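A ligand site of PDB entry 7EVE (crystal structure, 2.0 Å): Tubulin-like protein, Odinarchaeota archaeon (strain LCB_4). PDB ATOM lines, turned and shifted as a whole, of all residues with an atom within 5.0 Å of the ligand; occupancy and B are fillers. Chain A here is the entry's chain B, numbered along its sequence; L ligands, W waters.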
ATOM      1  N   VAL A  11     -26.669   4.449  -1.596  1.00  0.00           N
ATOM      2  CA  VAL A  11     -25.919   3.198  -1.568  1.00  0.00           C
ATOM      3  C   VAL A  11     -25.795   2.666  -2.995  1.00  0.00           C
ATOM      4  O   VAL A  11     -26.766   2.676  -3.755  1.00  0.00           O
ATOM      5  CB  VAL A  11     -26.599   2.150  -0.659  1.00  0.00           C
ATOM      6  CG1 VAL A  11     -25.622   1.033  -0.327  1.00  0.00           C
ATOM      7  CG2 VAL A  11     -27.122   2.803   0.607  1.00  0.00           C
ATOM      8  N   GLY A  12     -24.600   2.189  -3.333  1.00  0.00           N
ATOM      9  CA  GLY A  12     -24.360   1.613  -4.644  1.00  0.00           C
ATOM     10  C   GLY A  12     -24.235   2.661  -5.738  1.00  0.00           C
ATOM     11  O   GLY A  12     -24.396   3.864  -5.520  1.00  0.00           O
ATOM     12  N   GLN A  13     -23.945   2.172  -6.941  1.00  0.00           N
ATOM     13  CA  GLN A  13     -23.788   3.074  -8.084  1.00  0.00           C
ATOM     14  C   GLN A  13     -25.096   3.800  -8.392  1.00  0.00           C
ATOM     15  O   GLN A  13     -25.105   5.030  -8.540  1.00  0.00           O
ATOM     16  CB  GLN A  13     -23.314   2.296  -9.311  1.00  0.00           C
ATOM     17  CG  GLN A  13     -23.325   3.108 -10.589  1.00  0.00           C
ATOM     18  CD  GLN A  13     -22.454   2.528 -11.680  1.00  0.00           C
ATOM     19  OE1 GLN A  13     -22.052   1.363 -11.618  1.00  0.00           O
ATOM     20  NE2 GLN A  13     -22.132   3.338 -12.686  1.00  0.00           N
ATOM     21  N   GLY A  14     -26.198   3.059  -8.485  1.00  0.00           N
ATOM     22  CA  GLY A  14     -27.467   3.685  -8.796  1.00  0.00           C
ATOM     23  C   GLY A  14     -27.909   4.672  -7.723  1.00  0.00           C
ATOM     24  O   GLY A  14     -28.315   5.791  -8.036  1.00  0.00           O
ATOM     25  N   GLY A  15     -27.809   4.274  -6.458  1.00  0.00           N
ATOM     26  CA  GLY A  15     -28.250   5.139  -5.378  1.00  0.00           C
ATOM     27  C   GLY A  15     -27.502   6.460  -5.345  1.00  0.00           C
ATOM     28  O   GLY A  15     -28.078   7.503  -5.014  1.00  0.00           O
ATOM     29  N   GLN A  17     -25.796   7.819  -8.081  1.00  0.00           N
ATOM     30  CA  GLN A  17     -26.058   8.552  -9.318  1.00  0.00           C
ATOM     31  C   GLN A  17     -27.425   9.235  -9.271  1.00  0.00           C
ATOM     32  O   GLN A  17     -27.566  10.374  -9.730  1.00  0.00           O
ATOM     33  CB  GLN A  17     -25.960   7.611 -10.519  1.00  0.00           C
ATOM     34  CG  GLN A  17     -24.538   7.170 -10.822  1.00  0.00           C
ATOM     35  CD  GLN A  17     -24.451   6.188 -11.974  1.00  0.00           C
ATOM     36  OE1 GLN A  17     -23.404   6.023 -12.593  1.00  0.00           O
ATOM     37  NE2 GLN A  17     -25.566   5.517 -12.267  1.00  0.00           N
ATOM     38  N   ILE A  18     -28.428   8.549  -8.709  1.00  0.00           N
ATOM     39  CA  ILE A  18     -29.712   9.199  -8.459  1.00  0.00           C
ATOM     40  C   ILE A  18     -29.536  10.362  -7.481  1.00  0.00           C
ATOM     41  O   ILE A  18     -30.249  11.366  -7.568  1.00  0.00           O
ATOM     42  CB  ILE A  18     -30.730   8.168  -7.929  1.00  0.00           C
ATOM     43  CG1 ILE A  18     -30.977   7.079  -8.966  1.00  0.00           C
ATOM     44  CG2 ILE A  18     -32.035   8.833  -7.540  1.00  0.00           C
ATOM     45  CD1 ILE A  18     -31.608   5.825  -8.393  1.00  0.00           C
ATOM     46  N   ASP A  69     -20.798   3.306  -0.876  1.00  0.00           N
ATOM     47  CA  ASP A  69     -20.638   2.322  -1.936  1.00  0.00           C
ATOM     48  C   ASP A  69     -19.521   1.376  -1.555  1.00  0.00           C
ATOM     49  O   ASP A  69     -18.637   1.696  -0.756  1.00  0.00           O
ATOM     50  CB  ASP A  69     -20.344   2.980  -3.284  1.00  0.00           C
ATOM     51  CG  ASP A  69     -20.670   2.082  -4.454  1.00  0.00           C
ATOM     52  OD1 ASP A  69     -20.706   0.847  -4.265  1.00  0.00           O
ATOM     53  OD2 ASP A  69     -20.887   2.599  -5.562  1.00  0.00           O
ATOM     54  N   ALA A 100     -19.336  -5.725  -4.394  1.00  0.00           N
ATOM     55  CA  ALA A 100     -20.305  -6.767  -4.072  1.00  0.00           C
ATOM     56  C   ALA A 100     -20.509  -7.776  -5.194  1.00  0.00           C
ATOM     57  O   ALA A 100     -21.110  -8.820  -4.944  1.00  0.00           O
ATOM     58  CB  ALA A 100     -21.647  -6.137  -3.700  1.00  0.00           C
ATOM     59  N   ASN A 102     -22.509  -7.912  -7.658  1.00  0.00           N
ATOM     60  CA  ASN A 102     -23.931  -8.158  -7.921  1.00  0.00           C
ATOM     61  C   ASN A 102     -24.500  -9.272  -7.048  1.00  0.00           C
ATOM     62  O   ASN A 102     -25.480  -9.916  -7.416  1.00  0.00           O
ATOM     63  CB  ASN A 102     -24.180  -8.463  -9.396  1.00  0.00           C
ATOM     64  CG  ASN A 102     -24.067  -7.236 -10.282  1.00  0.00           C
ATOM     65  OD1 ASN A 102     -23.786  -6.136  -9.791  1.00  0.00           O
ATOM     66  ND2 ASN A 102     -24.272  -7.412 -11.577  1.00  0.00           N
ATOM     67  N   THR A 138     -30.722   0.690  -5.664  1.00  0.00           N
ATOM     68  CA  THR A 138     -31.316  -0.252  -6.603  1.00  0.00           C
ATOM     69  C   THR A 138     -31.418  -1.622  -5.949  1.00  0.00           C
ATOM     70  O   THR A 138     -30.722  -1.927  -4.977  1.00  0.00           O
ATOM     71  CB  THR A 138     -30.487  -0.338  -7.886  1.00  0.00           C
ATOM     72  OG1 THR A 138     -29.275  -1.058  -7.625  1.00  0.00           O
ATOM     73  CG2 THR A 138     -30.148   1.050  -8.412  1.00  0.00           C
ATOM     74  N   GLY A 140     -31.500  -4.629  -8.009  1.00  0.00           N
ATOM     75  CA  GLY A 140     -30.992  -5.675  -8.879  1.00  0.00           C
ATOM     76  C   GLY A 140     -29.523  -5.977  -8.739  1.00  0.00           C
ATOM     77  O   GLY A 140     -29.054  -7.043  -9.142  1.00  0.00           O
ATOM     78  N   GLY A 141     -28.769  -5.051  -8.149  1.00  0.00           N
ATOM     79  CA  GLY A 141     -27.335  -5.194  -7.977  1.00  0.00           C
ATOM     80  C   GLY A 141     -26.951  -5.829  -6.662  1.00  0.00           C
ATOM     81  O   GLY A 141     -27.705  -6.629  -6.086  1.00  0.00           O
ATOM     82  N   GLY A 142     -25.779  -5.455  -6.156  1.00  0.00           N
ATOM     83  CA  GLY A 142     -25.249  -6.070  -4.956  1.00  0.00           C
ATOM     84  C   GLY A 142     -25.086  -5.131  -3.781  1.00  0.00           C
ATOM     85  O   GLY A 142     -25.487  -5.469  -2.661  1.00  0.00           O
ATOM     86  N   THR A 143     -24.504  -3.951  -4.013  1.00  0.00           N
ATOM     87  CA  THR A 143     -24.285  -3.014  -2.920  1.00  0.00           C
ATOM     88  C   THR A 143     -25.585  -2.303  -2.530  1.00  0.00           C
ATOM     89  O   THR A 143     -25.948  -2.264  -1.356  1.00  0.00           O
ATOM     90  CB  THR A 143     -23.218  -1.992  -3.304  1.00  0.00           C
ATOM     91  OG1 THR A 143     -21.977  -2.672  -3.544  1.00  0.00           O
ATOM     92  CG2 THR A 143     -23.013  -0.984  -2.182  1.00  0.00           C
ATOM     93  N   GLY A 144     -26.294  -1.744  -3.520  1.00  0.00           N
ATOM     94  CA  GLY A 144     -27.571  -1.111  -3.222  1.00  0.00           C
ATOM     95  C   GLY A 144     -28.571  -2.081  -2.647  1.00  0.00           C
ATOM     96  O   GLY A 144     -29.368  -1.725  -1.772  1.00  0.00           O
ATOM     97  N   SER A 145     -28.549  -3.334  -3.104  1.00  0.00           N
ATOM     98  CA  SER A 145     -29.474  -4.332  -2.594  1.00  0.00           C
ATOM     99  C   SER A 145     -29.058  -4.855  -1.223  1.00  0.00           C
ATOM    100  O   SER A 145     -29.851  -4.832  -0.283  1.00  0.00           O
ATOM    101  CB  SER A 145     -29.591  -5.488  -3.595  1.00  0.00           C
ATOM    102  OG  SER A 145     -28.342  -6.137  -3.773  1.00  0.00           O
ATOM    103  N   VAL A 169     -35.085   0.890  -6.779  1.00  0.00           N
ATOM    104  CA  VAL A 169     -35.159   0.792  -8.233  1.00  0.00           C
ATOM    105  C   VAL A 169     -35.210  -0.679  -8.612  1.00  0.00           C
ATOM    106  O   VAL A 169     -34.245  -1.420  -8.384  1.00  0.00           O
ATOM    107  CB  VAL A 169     -33.973   1.495  -8.917  1.00  0.00           C
ATOM    108  CG1 VAL A 169     -34.099   1.397 -10.428  1.00  0.00           C
ATOM    109  CG2 VAL A 169     -33.891   2.944  -8.469  1.00  0.00           C
ATOM    110  N   PRO A 171     -35.372  -3.851 -11.370  1.00  0.00           N
ATOM    111  CA  PRO A 171     -34.784  -4.098 -12.698  1.00  0.00           C
ATOM    112  C   PRO A 171     -35.803  -3.871 -13.802  1.00  0.00           C
ATOM    113  O   PRO A 171     -37.018  -3.882 -13.584  1.00  0.00           O
ATOM    114  CB  PRO A 171     -34.354  -5.564 -12.629  1.00  0.00           C
ATOM    115  CG  PRO A 171     -34.306  -5.900 -11.173  1.00  0.00           C
ATOM    116  CD  PRO A 171     -35.366  -5.065 -10.533  1.00  0.00           C
ATOM    117  N   ASP A 176     -31.229  -6.408 -16.591  1.00  0.00           N
ATOM    118  CA  ASP A 176     -29.861  -6.211 -17.047  1.00  0.00           C
ATOM    119  C   ASP A 176     -28.843  -6.768 -16.057  1.00  0.00           C
ATOM    120  O   ASP A 176     -27.648  -6.486 -16.193  1.00  0.00           O
ATOM    121  CB  ASP A 176     -29.590  -4.726 -17.319  1.00  0.00           C
ATOM    122  CG  ASP A 176     -29.748  -3.865 -16.082  1.00  0.00           C
ATOM    123  OD1 ASP A 176     -30.601  -4.192 -15.236  1.00  0.00           O
ATOM    124  OD2 ASP A 176     -29.019  -2.862 -15.969  1.00  0.00           O
ATOM    125  N   VAL A 177     -29.300  -7.520 -15.064  1.00  0.00           N
ATOM    126  CA  VAL A 177     -28.456  -8.285 -14.153  1.00  0.00           C
ATOM    127  C   VAL A 177     -29.126  -9.635 -13.956  1.00  0.00           C
ATOM    128  O   VAL A 177     -30.243  -9.703 -13.447  1.00  0.00           O
ATOM    129  CB  VAL A 177     -28.246  -7.585 -12.800  1.00  0.00           C
ATOM    130  CG1 VAL A 177     -27.472  -8.484 -11.853  1.00  0.00           C
ATOM    131  CG2 VAL A 177     -27.532  -6.254 -12.975  1.00  0.00           C
ATOM    132  N   ASN A 203     -36.554   0.916 -14.595  1.00  0.00           N
ATOM    133  CA  ASN A 203     -35.997   1.707 -15.688  1.00  0.00           C
ATOM    134  C   ASN A 203     -36.846   1.618 -16.954  1.00  0.00           C
ATOM    135  O   ASN A 203     -36.800   2.538 -17.780  1.00  0.00           O
ATOM    136  CB  ASN A 203     -34.560   1.268 -15.974  1.00  0.00           C
ATOM    137  CG  ASN A 203     -33.622   1.600 -14.832  1.00  0.00           C
ATOM    138  OD1 ASN A 203     -33.899   2.471 -14.016  1.00  0.00           O
ATOM    139  ND2 ASN A 203     -32.494   0.890 -14.769  1.00  0.00           N
ATOM    140  N   LEU A 206     -39.372   4.368 -16.511  1.00  0.00           N
ATOM    141  CA  LEU A 206     -38.676   5.652 -16.535  1.00  0.00           C
ATOM    142  C   LEU A 206     -38.223   6.002 -17.947  1.00  0.00           C
ATOM    143  O   LEU A 206     -38.355   7.159 -18.370  1.00  0.00           O
ATOM    144  CB  LEU A 206     -37.482   5.619 -15.585  1.00  0.00           C
ATOM    145  CG  LEU A 206     -37.780   5.466 -14.089  1.00  0.00           C
ATOM    146  CD1 LEU A 206     -36.482   5.458 -13.281  1.00  0.00           C
ATOM    147  CD2 LEU A 206     -38.708   6.575 -13.605  1.00  0.00           C
ATOM    148  N   PHE A 222     -27.429   8.326 -17.073  1.00  0.00           N
ATOM    149  CA  PHE A 222     -28.577   8.122 -16.194  1.00  0.00           C
ATOM    150  C   PHE A 222     -29.129   9.419 -15.636  1.00  0.00           C
ATOM    151  O   PHE A 222     -30.198   9.403 -15.006  1.00  0.00           O
ATOM    152  CB  PHE A 222     -28.202   7.175 -15.040  1.00  0.00           C
ATOM    153  CG  PHE A 222     -28.454   5.725 -15.345  1.00  0.00           C
ATOM    154  CD1 PHE A 222     -29.733   5.280 -15.643  1.00  0.00           C
ATOM    155  CD2 PHE A 222     -27.424   4.801 -15.328  1.00  0.00           C
ATOM    156  CE1 PHE A 222     -29.975   3.945 -15.928  1.00  0.00           C
ATOM    157  CE2 PHE A 222     -27.656   3.472 -15.605  1.00  0.00           C
ATOM    158  CZ  PHE A 222     -28.940   3.043 -15.907  1.00  0.00           C
ATOM    159  N   LEU A 225     -32.358  10.054 -16.892  1.00  0.00           N
ATOM    160  CA  LEU A 225     -33.329   9.112 -16.344  1.00  0.00           C
ATOM    161  C   LEU A 225     -33.646   9.377 -14.881  1.00  0.00           C
ATOM    162  O   LEU A 225     -34.819   9.360 -14.490  1.00  0.00           O
ATOM    163  CB  LEU A 225     -32.820   7.676 -16.483  1.00  0.00           C
ATOM    164  CG  LEU A 225     -33.429   6.757 -17.533  1.00  0.00           C
ATOM    165  CD1 LEU A 225     -33.209   5.293 -17.154  1.00  0.00           C
ATOM    166  CD2 LEU A 225     -34.909   7.054 -17.727  1.00  0.00           C
ATOM    167  N   ASN A 226     -32.621   9.634 -14.073  1.00  0.00           N
ATOM    168  CA  ASN A 226     -32.777   9.723 -12.622  1.00  0.00           C
ATOM    169  C   ASN A 226     -33.458  11.013 -12.168  1.00  0.00           C
ATOM    170  O   ASN A 226     -33.805  11.113 -10.993  1.00  0.00           O
ATOM    171  CB  ASN A 226     -31.417   9.585 -11.938  1.00  0.00           C
ATOM    172  CG  ASN A 226     -30.783   8.232 -12.186  1.00  0.00           C
ATOM    173  OD1 ASN A 226     -31.468   7.246 -12.462  1.00  0.00           O
ATOM    174  ND2 ASN A 226     -29.462   8.181 -12.095  1.00  0.00           N
ATOM    175  N   ILE A 229     -36.817  10.364 -10.513  1.00  0.00           N
ATOM    176  CA  ILE A 229     -36.764   9.938  -9.121  1.00  0.00           C
ATOM    177  C   ILE A 229     -36.537  11.139  -8.211  1.00  0.00           C
ATOM    178  O   ILE A 229     -37.146  11.253  -7.131  1.00  0.00           O
ATOM    179  CB  ILE A 229     -35.682   8.869  -8.934  1.00  0.00           C
ATOM    180  CG1 ILE A 229     -35.873   7.741  -9.951  1.00  0.00           C
ATOM    181  CG2 ILE A 229     -35.711   8.318  -7.511  1.00  0.00           C
ATOM    182  CD1 ILE A 229     -34.784   6.691  -9.920  1.00  0.00           C
HETATM  183  P1  LIG L   1     -24.595  -1.862  -6.940  1.00  0.00           P
HETATM  184  O1  LIG L   1     -23.549  -0.764  -6.973  1.00  0.00           O
HETATM  185  O2  LIG L   1     -25.773  -1.445  -6.094  1.00  0.00           O
HETATM  186  O3  LIG L   1     -23.966  -3.100  -6.354  1.00  0.00           O
HETATM  187  O4  LIG L   1     -25.069  -2.204  -8.441  1.00  0.00           O
HETATM  188  P2  LIG L   1     -26.052  -1.243  -9.286  1.00  0.00           P
HETATM  189  O5  LIG L   1     -25.382  -0.801 -10.573  1.00  0.00           O
HETATM  190  O6  LIG L   1     -26.472  -0.039  -8.474  1.00  0.00           O
HETATM  191  O7  LIG L   1     -27.303  -2.197  -9.607  1.00  0.00           O
HETATM  192  C1  LIG L   1     -27.592  -2.560 -10.957  1.00  0.00           C
HETATM  193  C2  LIG L   1     -29.076  -2.382 -11.220  1.00  0.00           C
HETATM  194  O8  LIG L   1     -29.418  -1.038 -10.878  1.00  0.00           O
HETATM  195  C3  LIG L   1     -29.370  -2.533 -12.696  1.00  0.00           C
HETATM  196  O9  LIG L   1     -30.679  -3.066 -12.882  1.00  0.00           O
HETATM  197  C4  LIG L   1     -29.333  -1.116 -13.226  1.00  0.00           C
HETATM  198  O10 LIG L   1     -30.210  -0.965 -14.348  1.00  0.00           O
HETATM  199  C5  LIG L   1     -29.787  -0.291 -12.040  1.00  0.00           C
HETATM  200  N1  LIG L   1     -29.109   1.017 -12.013  1.00  0.00           N
HETATM  201  C6  LIG L   1     -27.795   1.216 -11.842  1.00  0.00           C
HETATM  202  N2  LIG L   1     -27.490   2.543 -11.872  1.00  0.00           N
HETATM  203  C7  LIG L   1     -28.646   3.212 -12.037  1.00  0.00           C
HETATM  204  C8  LIG L   1     -29.058   4.628 -12.130  1.00  0.00           C
HETATM  205  O11 LIG L   1     -28.209   5.547 -12.062  1.00  0.00           O
HETATM  206  N3  LIG L   1     -30.357   4.908 -12.307  1.00  0.00           N
HETATM  207  C9  LIG L   1     -31.287   3.936 -12.378  1.00  0.00           C
HETATM  208  N4  LIG L   1     -32.588   4.291 -12.554  1.00  0.00           N
HETATM  209  N5  LIG L   1     -30.987   2.611 -12.298  1.00  0.00           N
HETATM  210  C10 LIG L   1     -29.713   2.202 -12.127  1.00  0.00           C
HETATM  211  O   HOH W   1     -27.561   1.335  -5.913  1.00  0.00           O
HETATM  212  O   HOH W   2     -32.538  -2.838 -10.471  1.00  0.00           O
HETATM  213  O   HOH W   3     -24.357  -2.972 -12.193  1.00  0.00           O
HETATM  214  O   HOH W   4     -27.814  -2.856  -5.944  1.00  0.00           O
HETATM  215  O   HOH W   5     -22.182  -5.547  -6.874  1.00  0.00           O
HETATM  216  O   HOH W   6     -32.607  -2.030 -15.333  1.00  0.00           O
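Merely in contact with the ligand: Gly 12, Gly 141, Val 169 and Phe 222. Hydrophobic or aromatic side chains that line the ligand: Val 169 and Phe 222. Of the 27 residues printed, 14 come within 4 Å of the ligand. The nearest printed residue that does not touch the ligand is Ile 18 (4.03 Å).
The backbone NH (N) of Gln 13 is in hydrogen-bond range of the side-chain carboxylate (OD2) of Asp 69 (3.4 Å). The side-chain hydroxyl (OG) of Ser 145 is in hydrogen-bond range of the backbone carbonyl oxygen (O) of Gly 141, 2.4 Å away. The backbone carbonyl oxygen (O) of Thr 138 is in hydrogen-bond range of the backbone NH (N) of Ser 145, at 3.2 Å. The backbone carbonyl oxygen (O) of Phe 222 lies close to the side-chain amide nitrogen (ND2) of Asn 226 (3.2 Å). The side-chain amide oxygen of Gln 17 is in hydrogen-bond range of the side-chain amide nitrogen of Gln 13 (3.0 Å). OG of Ser 145 is in hydrogen-bond range of O of Gly 142 (3.1 Å).
An oxygen (O3) of the ligand lies within hydrogen-bond range of the backbone NH of Thr 143 (2.5 Å). O2 of the ligand sits at hydrogen-bond distance from N of Gly 144, 2.6 Å away. The backbone NH (N) of Gln 13 lies within hydrogen-bond range of an oxygen (O1) of the ligand, at 3.0 Å. An oxygen (O6) of the ligand lies within hydrogen-bond range of the backbone NH of Gly 14 (3.1 Å). An oxygen (O3) of the ligand sits at hydrogen-bond distance from the backbone NH (N) of Gly 142 (3.0 Å). NE2 of Gln 17 sits at hydrogen-bond distance from O11 of the ligand (2.7 Å). The side-chain amide oxygen of Asn 203 sits at hydrogen-bond distance from a nitrogen (N4) of the ligand. An oxygen (O7) of the ligand sits at hydrogen-bond distance from the side-chain hydroxyl (OG1) of Thr 138, 3.0 Å away. A nitrogen (N3) of the ligand lies within hydrogen-bond range of the side-chain amide oxygen (OD1) of Asn 226, 2.6 Å away. An oxygen (O3) of the ligand lies close to the side-chain hydroxyl (OG1) of Thr 143 (3.5 Å). The side-chain carboxylate (OD1) of Asp 176 lies within hydrogen-bond range of an oxygen (O9) of the ligand (2.6 Å).
Water W6 lies within hydrogen-bond range of an oxygen (O10) of the ligand, the side-chain carboxylate of Asp 176 and the side-chain amide nitrogen of Asn 203. Water W2 lies within hydrogen-bond range of the backbone carbonyl oxygen (O) of Val 169 (3.0 Å), an oxygen (O9) of the ligand (3.1 Å) and the backbone NH (N) of Gly 140 (3.2 Å). Water W5 bridges N of Asn 102 (2.5 Å) and O3 of the ligand (3.1 Å).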
